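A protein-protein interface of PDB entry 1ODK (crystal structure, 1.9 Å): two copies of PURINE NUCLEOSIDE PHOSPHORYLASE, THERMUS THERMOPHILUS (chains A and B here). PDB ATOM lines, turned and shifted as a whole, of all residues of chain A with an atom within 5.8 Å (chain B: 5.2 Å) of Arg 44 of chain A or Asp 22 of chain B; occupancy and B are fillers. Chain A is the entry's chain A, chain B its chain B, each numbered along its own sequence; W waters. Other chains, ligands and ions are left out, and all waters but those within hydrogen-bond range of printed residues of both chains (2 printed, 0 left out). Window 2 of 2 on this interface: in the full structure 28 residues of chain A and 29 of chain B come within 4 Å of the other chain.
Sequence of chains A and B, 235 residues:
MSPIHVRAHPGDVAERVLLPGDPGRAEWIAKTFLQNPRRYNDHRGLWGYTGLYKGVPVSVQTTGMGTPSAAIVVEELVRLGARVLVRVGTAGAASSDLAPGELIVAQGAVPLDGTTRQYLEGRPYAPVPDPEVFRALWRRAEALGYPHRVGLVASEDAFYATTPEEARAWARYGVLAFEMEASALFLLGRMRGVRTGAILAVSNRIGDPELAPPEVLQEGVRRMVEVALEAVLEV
Water W2 bridges N of Arg 44 of chain A and OD1 of Asp 22 of chain B. Water W1 lies within hydrogen-bond range of the backbone carbonyl oxygen of Gly 21 of chain B (2.8 Å) and the guanidinium group of Arg 44 of chain A (2.9 Å).
Met 65 of chain B touches His 5 of chain A. Gly 21 of chain B touches Arg 44 of chain A. Arg 44 of chain A touches Asp 22 of chain B (CA to OD1, 3.4 Å). Arg 44 of chain A touches Pro 23 of chain B. Met 65 of chain B touches Arg 44 of chain A (CG to NH1, 3.6 Å). N of Gly 45 of chain A touches CG of Pro 23 of chain B, at 3.6 Å. Leu 46 of chain A touches Met 65 of chain B (CD1 to CE, 3.7 Å).
Of the printed residues of chain B, His 5 of chain A touches Met 65. Of the printed residues of chain B, Arg 44 of chain A touches Gly 21 (3.98 Å), Asp 22 (3.4 Å), Pro 23 (3.3 Å) and Met 65 (3.6 Å). Of the printed residues of chain A, Gly 21 of chain B touches Arg 44 (3.98 Å). Asp 22 of chain B touches just one residue of chain A: Arg 44. Of the printed residues of chain A, Pro 23 of chain B touches Arg 44 (3.3 Å) and Gly 45 (3.6 Å). Of the printed residues of chain A, Met 65 of chain B touches His 5, Arg 44 and Leu 46. The nearest printed residue of chain B that does not touch Arg 44 of chain A is Thr 90 of chain B (4.1 Å). The nearest residue of chain A that does not touch Asp 22 of chain B is His 43 of chain A (4.04 Å).
ND2 of Asn 41 of chain A is in hydrogen-bond range of O of Leu 46 of chain A, at 2.8 Å. The side-chain carboxylate of Asp 22 of chain B sits at hydrogen-bond distance from the backbone NH of Gly 24 of chain B, 2.7 Å away.
No position is printed for both chains. Of the 7 pairs that touch across the chains among the printed residues, none has its exchanged pair printed and touching as well.
Of the 10 printed residues of chain B, 4 touch a printed residue of chain A. Hydrophobic or aromatic side chains of chain B within 4 Å of the printed part of chain A: Pro 23 and Met 65. Of the 8 printed residues of chain A, 4 touch a printed residue of chain B. Printed residues of chain A that touch a printed residue of chain B: His 5, Arg 44, Gly 45 and Leu 46. Hydrophobic or aromatic side chains of chain A within 4 Å of the printed part of chain B: His 5 and Leu 46. Among the printed residues, no Asp or Glu carboxylate lies within 4 Å of a Lys or Arg side-chain nitrogen of the other chain.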
ATOM      1  N   ILE A   4     -16.026 -12.772  34.991  1.00  0.00           N
ATOM      2  CA  ILE A   4     -17.195 -12.272  34.282  1.00  0.00           C
ATOM      3  C   ILE A   4     -16.941 -11.178  33.239  1.00  0.00           C
ATOM      4  O   ILE A   4     -17.504 -11.226  32.144  1.00  0.00           O
ATOM      5  CB  ILE A   4     -18.249 -11.762  35.292  1.00  0.00           C
ATOM      6  CG1 ILE A   4     -18.749 -12.934  36.142  1.00  0.00           C
ATOM      7  CG2 ILE A   4     -19.404 -11.104  34.563  1.00  0.00           C
ATOM      8  CD1 ILE A   4     -19.665 -12.529  37.280  1.00  0.00           C
ATOM      9  N   HIS A   5     -16.095 -10.202  33.559  1.00  0.00           N
ATOM     10  CA  HIS A   5     -15.842  -9.101  32.633  1.00  0.00           C
ATOM     11  C   HIS A   5     -14.539  -9.220  31.846  1.00  0.00           C
ATOM     12  O   HIS A   5     -14.520  -9.022  30.632  1.00  0.00           O
ATOM     13  CB  HIS A   5     -15.896  -7.775  33.397  1.00  0.00           C
ATOM     14  CG  HIS A   5     -17.121  -7.627  34.249  1.00  0.00           C
ATOM     15  ND1 HIS A   5     -17.260  -8.257  35.467  1.00  0.00           N
ATOM     16  CD2 HIS A   5     -18.282  -6.964  34.035  1.00  0.00           C
ATOM     17  CE1 HIS A   5     -18.453  -7.988  35.968  1.00  0.00           C
ATOM     18  NE2 HIS A   5     -19.094  -7.205  35.117  1.00  0.00           N
ATOM     19  N   ASN A  41      -7.870 -10.060  25.982  1.00  0.00           N
ATOM     20  CA  ASN A  41      -9.281  -9.749  26.203  1.00  0.00           C
ATOM     21  C   ASN A  41      -9.783  -8.528  25.459  1.00  0.00           C
ATOM     22  O   ASN A  41      -9.113  -7.498  25.417  1.00  0.00           O
ATOM     23  CB  ASN A  41      -9.578  -9.512  27.686  1.00  0.00           C
ATOM     24  CG  ASN A  41     -11.058  -9.230  27.942  1.00  0.00           C
ATOM     25  OD1 ASN A  41     -11.889 -10.132  27.856  1.00  0.00           O
ATOM     26  ND2 ASN A  41     -11.391  -7.972  28.238  1.00  0.00           N
ATOM     27  N   ASP A  42     -10.969  -8.644  24.870  1.00  0.00           N
ATOM     28  CA  ASP A  42     -11.573  -7.499  24.208  1.00  0.00           C
ATOM     29  C   ASP A  42     -13.040  -7.415  24.618  1.00  0.00           C
ATOM     30  O   ASP A  42     -13.773  -6.537  24.169  1.00  0.00           O
ATOM     31  CB  ASP A  42     -11.409  -7.565  22.681  1.00  0.00           C
ATOM     32  CG  ASP A  42     -12.114  -8.750  22.048  1.00  0.00           C
ATOM     33  OD1 ASP A  42     -11.848  -8.996  20.854  1.00  0.00           O
ATOM     34  OD2 ASP A  42     -12.925  -9.424  22.714  1.00  0.00           O
ATOM     35  N   HIS A  43     -13.455  -8.327  25.495  1.00  0.00           N
ATOM     36  CA  HIS A  43     -14.833  -8.345  25.982  1.00  0.00           C
ATOM     37  C   HIS A  43     -15.168  -7.024  26.675  1.00  0.00           C
ATOM     38  O   HIS A  43     -14.375  -6.513  27.465  1.00  0.00           O
ATOM     39  CB  HIS A  43     -15.045  -9.498  26.966  1.00  0.00           C
ATOM     40  CG  HIS A  43     -16.454  -9.608  27.461  1.00  0.00           C
ATOM     41  ND1 HIS A  43     -17.522  -9.837  26.616  1.00  0.00           N
ATOM     42  CD2 HIS A  43     -16.977  -9.483  28.704  1.00  0.00           C
ATOM     43  CE1 HIS A  43     -18.641  -9.845  27.319  1.00  0.00           C
ATOM     44  NE2 HIS A  43     -18.338  -9.631  28.586  1.00  0.00           N
ATOM     45  N   ARG A  44     -16.353  -6.492  26.374  1.00  0.00           N
ATOM     46  CA  ARG A  44     -16.831  -5.226  26.924  1.00  0.00           C
ATOM     47  C   ARG A  44     -15.927  -4.049  26.586  1.00  0.00           C
ATOM     48  O   ARG A  44     -16.058  -2.971  27.164  1.00  0.00           O
ATOM     49  CB  ARG A  44     -17.019  -5.324  28.445  1.00  0.00           C
ATOM     50  CG  ARG A  44     -18.394  -5.846  28.852  1.00  0.00           C
ATOM     51  CD  ARG A  44     -18.533  -5.989  30.363  1.00  0.00           C
ATOM     52  NE  ARG A  44     -19.869  -6.446  30.747  1.00  0.00           N
ATOM     53  CZ  ARG A  44     -20.946  -5.666  30.817  1.00  0.00           C
ATOM     54  NH1 ARG A  44     -20.863  -4.373  30.536  1.00  0.00           N
ATOM     55  NH2 ARG A  44     -22.117  -6.182  31.163  1.00  0.00           N
ATOM     56  N   GLY A  45     -15.017  -4.256  25.639  1.00  0.00           N
ATOM     57  CA  GLY A  45     -14.109  -3.193  25.242  1.00  0.00           C
ATOM     58  C   GLY A  45     -12.985  -2.977  26.238  1.00  0.00           C
ATOM     59  O   GLY A  45     -12.196  -2.039  26.103  1.00  0.00           O
ATOM     60  N   LEU A  46     -12.915  -3.843  27.243  1.00  0.00           N
ATOM     61  CA  LEU A  46     -11.874  -3.755  28.267  1.00  0.00           C
ATOM     62  C   LEU A  46     -10.601  -4.401  27.719  1.00  0.00           C
ATOM     63  O   LEU A  46     -10.146  -5.437  28.213  1.00  0.00           O
ATOM     64  CB  LEU A  46     -12.337  -4.477  29.535  1.00  0.00           C
ATOM     65  CG  LEU A  46     -13.587  -3.884  30.205  1.00  0.00           C
ATOM     66  CD1 LEU A  46     -14.169  -4.884  31.179  1.00  0.00           C
ATOM     67  CD2 LEU A  46     -13.230  -2.579  30.916  1.00  0.00           C
ATOM     68  N   PRO B  20     -26.876   0.664  26.076  1.00  0.00           N
ATOM     69  CA  PRO B  20     -26.405  -0.606  26.635  1.00  0.00           C
ATOM     70  C   PRO B  20     -25.082  -0.305  27.349  1.00  0.00           C
ATOM     71  O   PRO B  20     -24.458   0.714  27.073  1.00  0.00           O
ATOM     72  CB  PRO B  20     -26.220  -1.484  25.400  1.00  0.00           C
ATOM     73  CG  PRO B  20     -25.838  -0.486  24.330  1.00  0.00           C
ATOM     74  CD  PRO B  20     -26.761   0.683  24.605  1.00  0.00           C
ATOM     75  N   GLY B  21     -24.661  -1.161  28.274  1.00  0.00           N
ATOM     76  CA  GLY B  21     -23.405  -0.900  28.961  1.00  0.00           C
ATOM     77  C   GLY B  21     -22.217  -1.456  28.191  1.00  0.00           C
ATOM     78  O   GLY B  21     -21.128  -0.879  28.171  1.00  0.00           O
ATOM     79  N   ASP B  22     -22.455  -2.580  27.529  1.00  0.00           N
ATOM     80  CA  ASP B  22     -21.442  -3.301  26.758  1.00  0.00           C
ATOM     81  C   ASP B  22     -21.347  -2.845  25.288  1.00  0.00           C
ATOM     82  O   ASP B  22     -22.328  -2.901  24.549  1.00  0.00           O
ATOM     83  CB  ASP B  22     -21.789  -4.792  26.849  1.00  0.00           C
ATOM     84  CG  ASP B  22     -20.865  -5.675  26.042  1.00  0.00           C
ATOM     85  OD1 ASP B  22     -19.912  -5.172  25.407  1.00  0.00           O
ATOM     86  OD2 ASP B  22     -21.104  -6.898  26.054  1.00  0.00           O
ATOM     87  N   PRO B  23     -20.155  -2.400  24.847  1.00  0.00           N
ATOM     88  CA  PRO B  23     -19.982  -1.949  23.458  1.00  0.00           C
ATOM     89  C   PRO B  23     -20.253  -3.048  22.426  1.00  0.00           C
ATOM     90  O   PRO B  23     -20.681  -2.767  21.302  1.00  0.00           O
ATOM     91  CB  PRO B  23     -18.534  -1.457  23.432  1.00  0.00           C
ATOM     92  CG  PRO B  23     -17.870  -2.316  24.472  1.00  0.00           C
ATOM     93  CD  PRO B  23     -18.883  -2.308  25.586  1.00  0.00           C
ATOM     94  N   GLY B  24     -19.997  -4.296  22.807  1.00  0.00           N
ATOM     95  CA  GLY B  24     -20.250  -5.404  21.905  1.00  0.00           C
ATOM     96  C   GLY B  24     -21.748  -5.567  21.711  1.00  0.00           C
ATOM     97  O   GLY B  24     -22.212  -5.997  20.653  1.00  0.00           O
ATOM     98  N   ARG B  25     -22.509  -5.224  22.745  1.00  0.00           N
ATOM     99  CA  ARG B  25     -23.959  -5.319  22.682  1.00  0.00           C
ATOM    100  C   ARG B  25     -24.503  -4.160  21.847  1.00  0.00           C
ATOM    101  O   ARG B  25     -25.458  -4.325  21.084  1.00  0.00           O
ATOM    102  CB  ARG B  25     -24.542  -5.289  24.098  1.00  0.00           C
ATOM    103  CG  ARG B  25     -26.052  -5.422  24.177  1.00  0.00           C
ATOM    104  CD  ARG B  25     -26.441  -5.882  25.571  1.00  0.00           C
ATOM    105  NE  ARG B  25     -25.961  -7.239  25.825  1.00  0.00           N
ATOM    106  CZ  ARG B  25     -25.514  -7.676  26.999  1.00  0.00           C
ATOM    107  NH1 ARG B  25     -25.476  -6.858  28.045  1.00  0.00           N
ATOM    108  NH2 ARG B  25     -25.107  -8.933  27.127  1.00  0.00           N
ATOM    109  N   ALA B  26     -23.892  -2.987  21.990  1.00  0.00           N
ATOM    110  CA  ALA B  26     -24.316  -1.823  21.219  1.00  0.00           C
ATOM    111  C   ALA B  26     -24.188  -2.146  19.731  1.00  0.00           C
ATOM    112  O   ALA B  26     -25.097  -1.876  18.943  1.00  0.00           O
ATOM    113  CB  ALA B  26     -23.452  -0.617  21.562  1.00  0.00           C
ATOM    114  N   THR B  62     -22.958   3.197  23.920  1.00  0.00           N
ATOM    115  CA  THR B  62     -22.314   2.439  24.989  1.00  0.00           C
ATOM    116  C   THR B  62     -22.104   3.363  26.188  1.00  0.00           C
ATOM    117  O   THR B  62     -21.659   4.497  26.020  1.00  0.00           O
ATOM    118  CB  THR B  62     -20.933   1.932  24.529  1.00  0.00           C
ATOM    119  OG1 THR B  62     -21.092   1.084  23.388  1.00  0.00           O
ATOM    120  CG2 THR B  62     -20.233   1.175  25.648  1.00  0.00           C
ATOM    121  N   MET B  65     -19.414   0.605  32.378  1.00  0.00           N
ATOM    122  CA  MET B  65     -19.996   0.095  33.617  1.00  0.00           C
ATOM    123  C   MET B  65     -19.880   1.102  34.751  1.00  0.00           C
ATOM    124  O   MET B  65     -18.841   1.745  34.914  1.00  0.00           O
ATOM    125  CB  MET B  65     -19.295  -1.198  34.043  1.00  0.00           C
ATOM    126  CG  MET B  65     -19.248  -2.271  32.966  1.00  0.00           C
ATOM    127  SD  MET B  65     -18.365  -3.734  33.540  1.00  0.00           S
ATOM    128  CE  MET B  65     -16.683  -3.213  33.384  1.00  0.00           C
ATOM    129  N   THR B  90     -28.060  -5.710  31.856  1.00  0.00           N
ATOM    130  CA  THR B  90     -28.228  -6.924  32.633  1.00  0.00           C
ATOM    131  C   THR B  90     -28.278  -6.595  34.117  1.00  0.00           C
ATOM    132  O   THR B  90     -27.850  -5.521  34.542  1.00  0.00           O
ATOM    133  CB  THR B  90     -27.069  -7.885  32.384  1.00  0.00           C
ATOM    134  OG1 THR B  90     -25.836  -7.181  32.566  1.00  0.00           O
ATOM    135  CG2 THR B  90     -27.133  -8.438  30.965  1.00  0.00           C
HETATM  136  O   HOH W   1     -19.054  -2.369  29.406  1.00  0.00           O
HETATM  137  O   HOH W   2     -18.087  -7.063  24.306  1.00  0.00           O
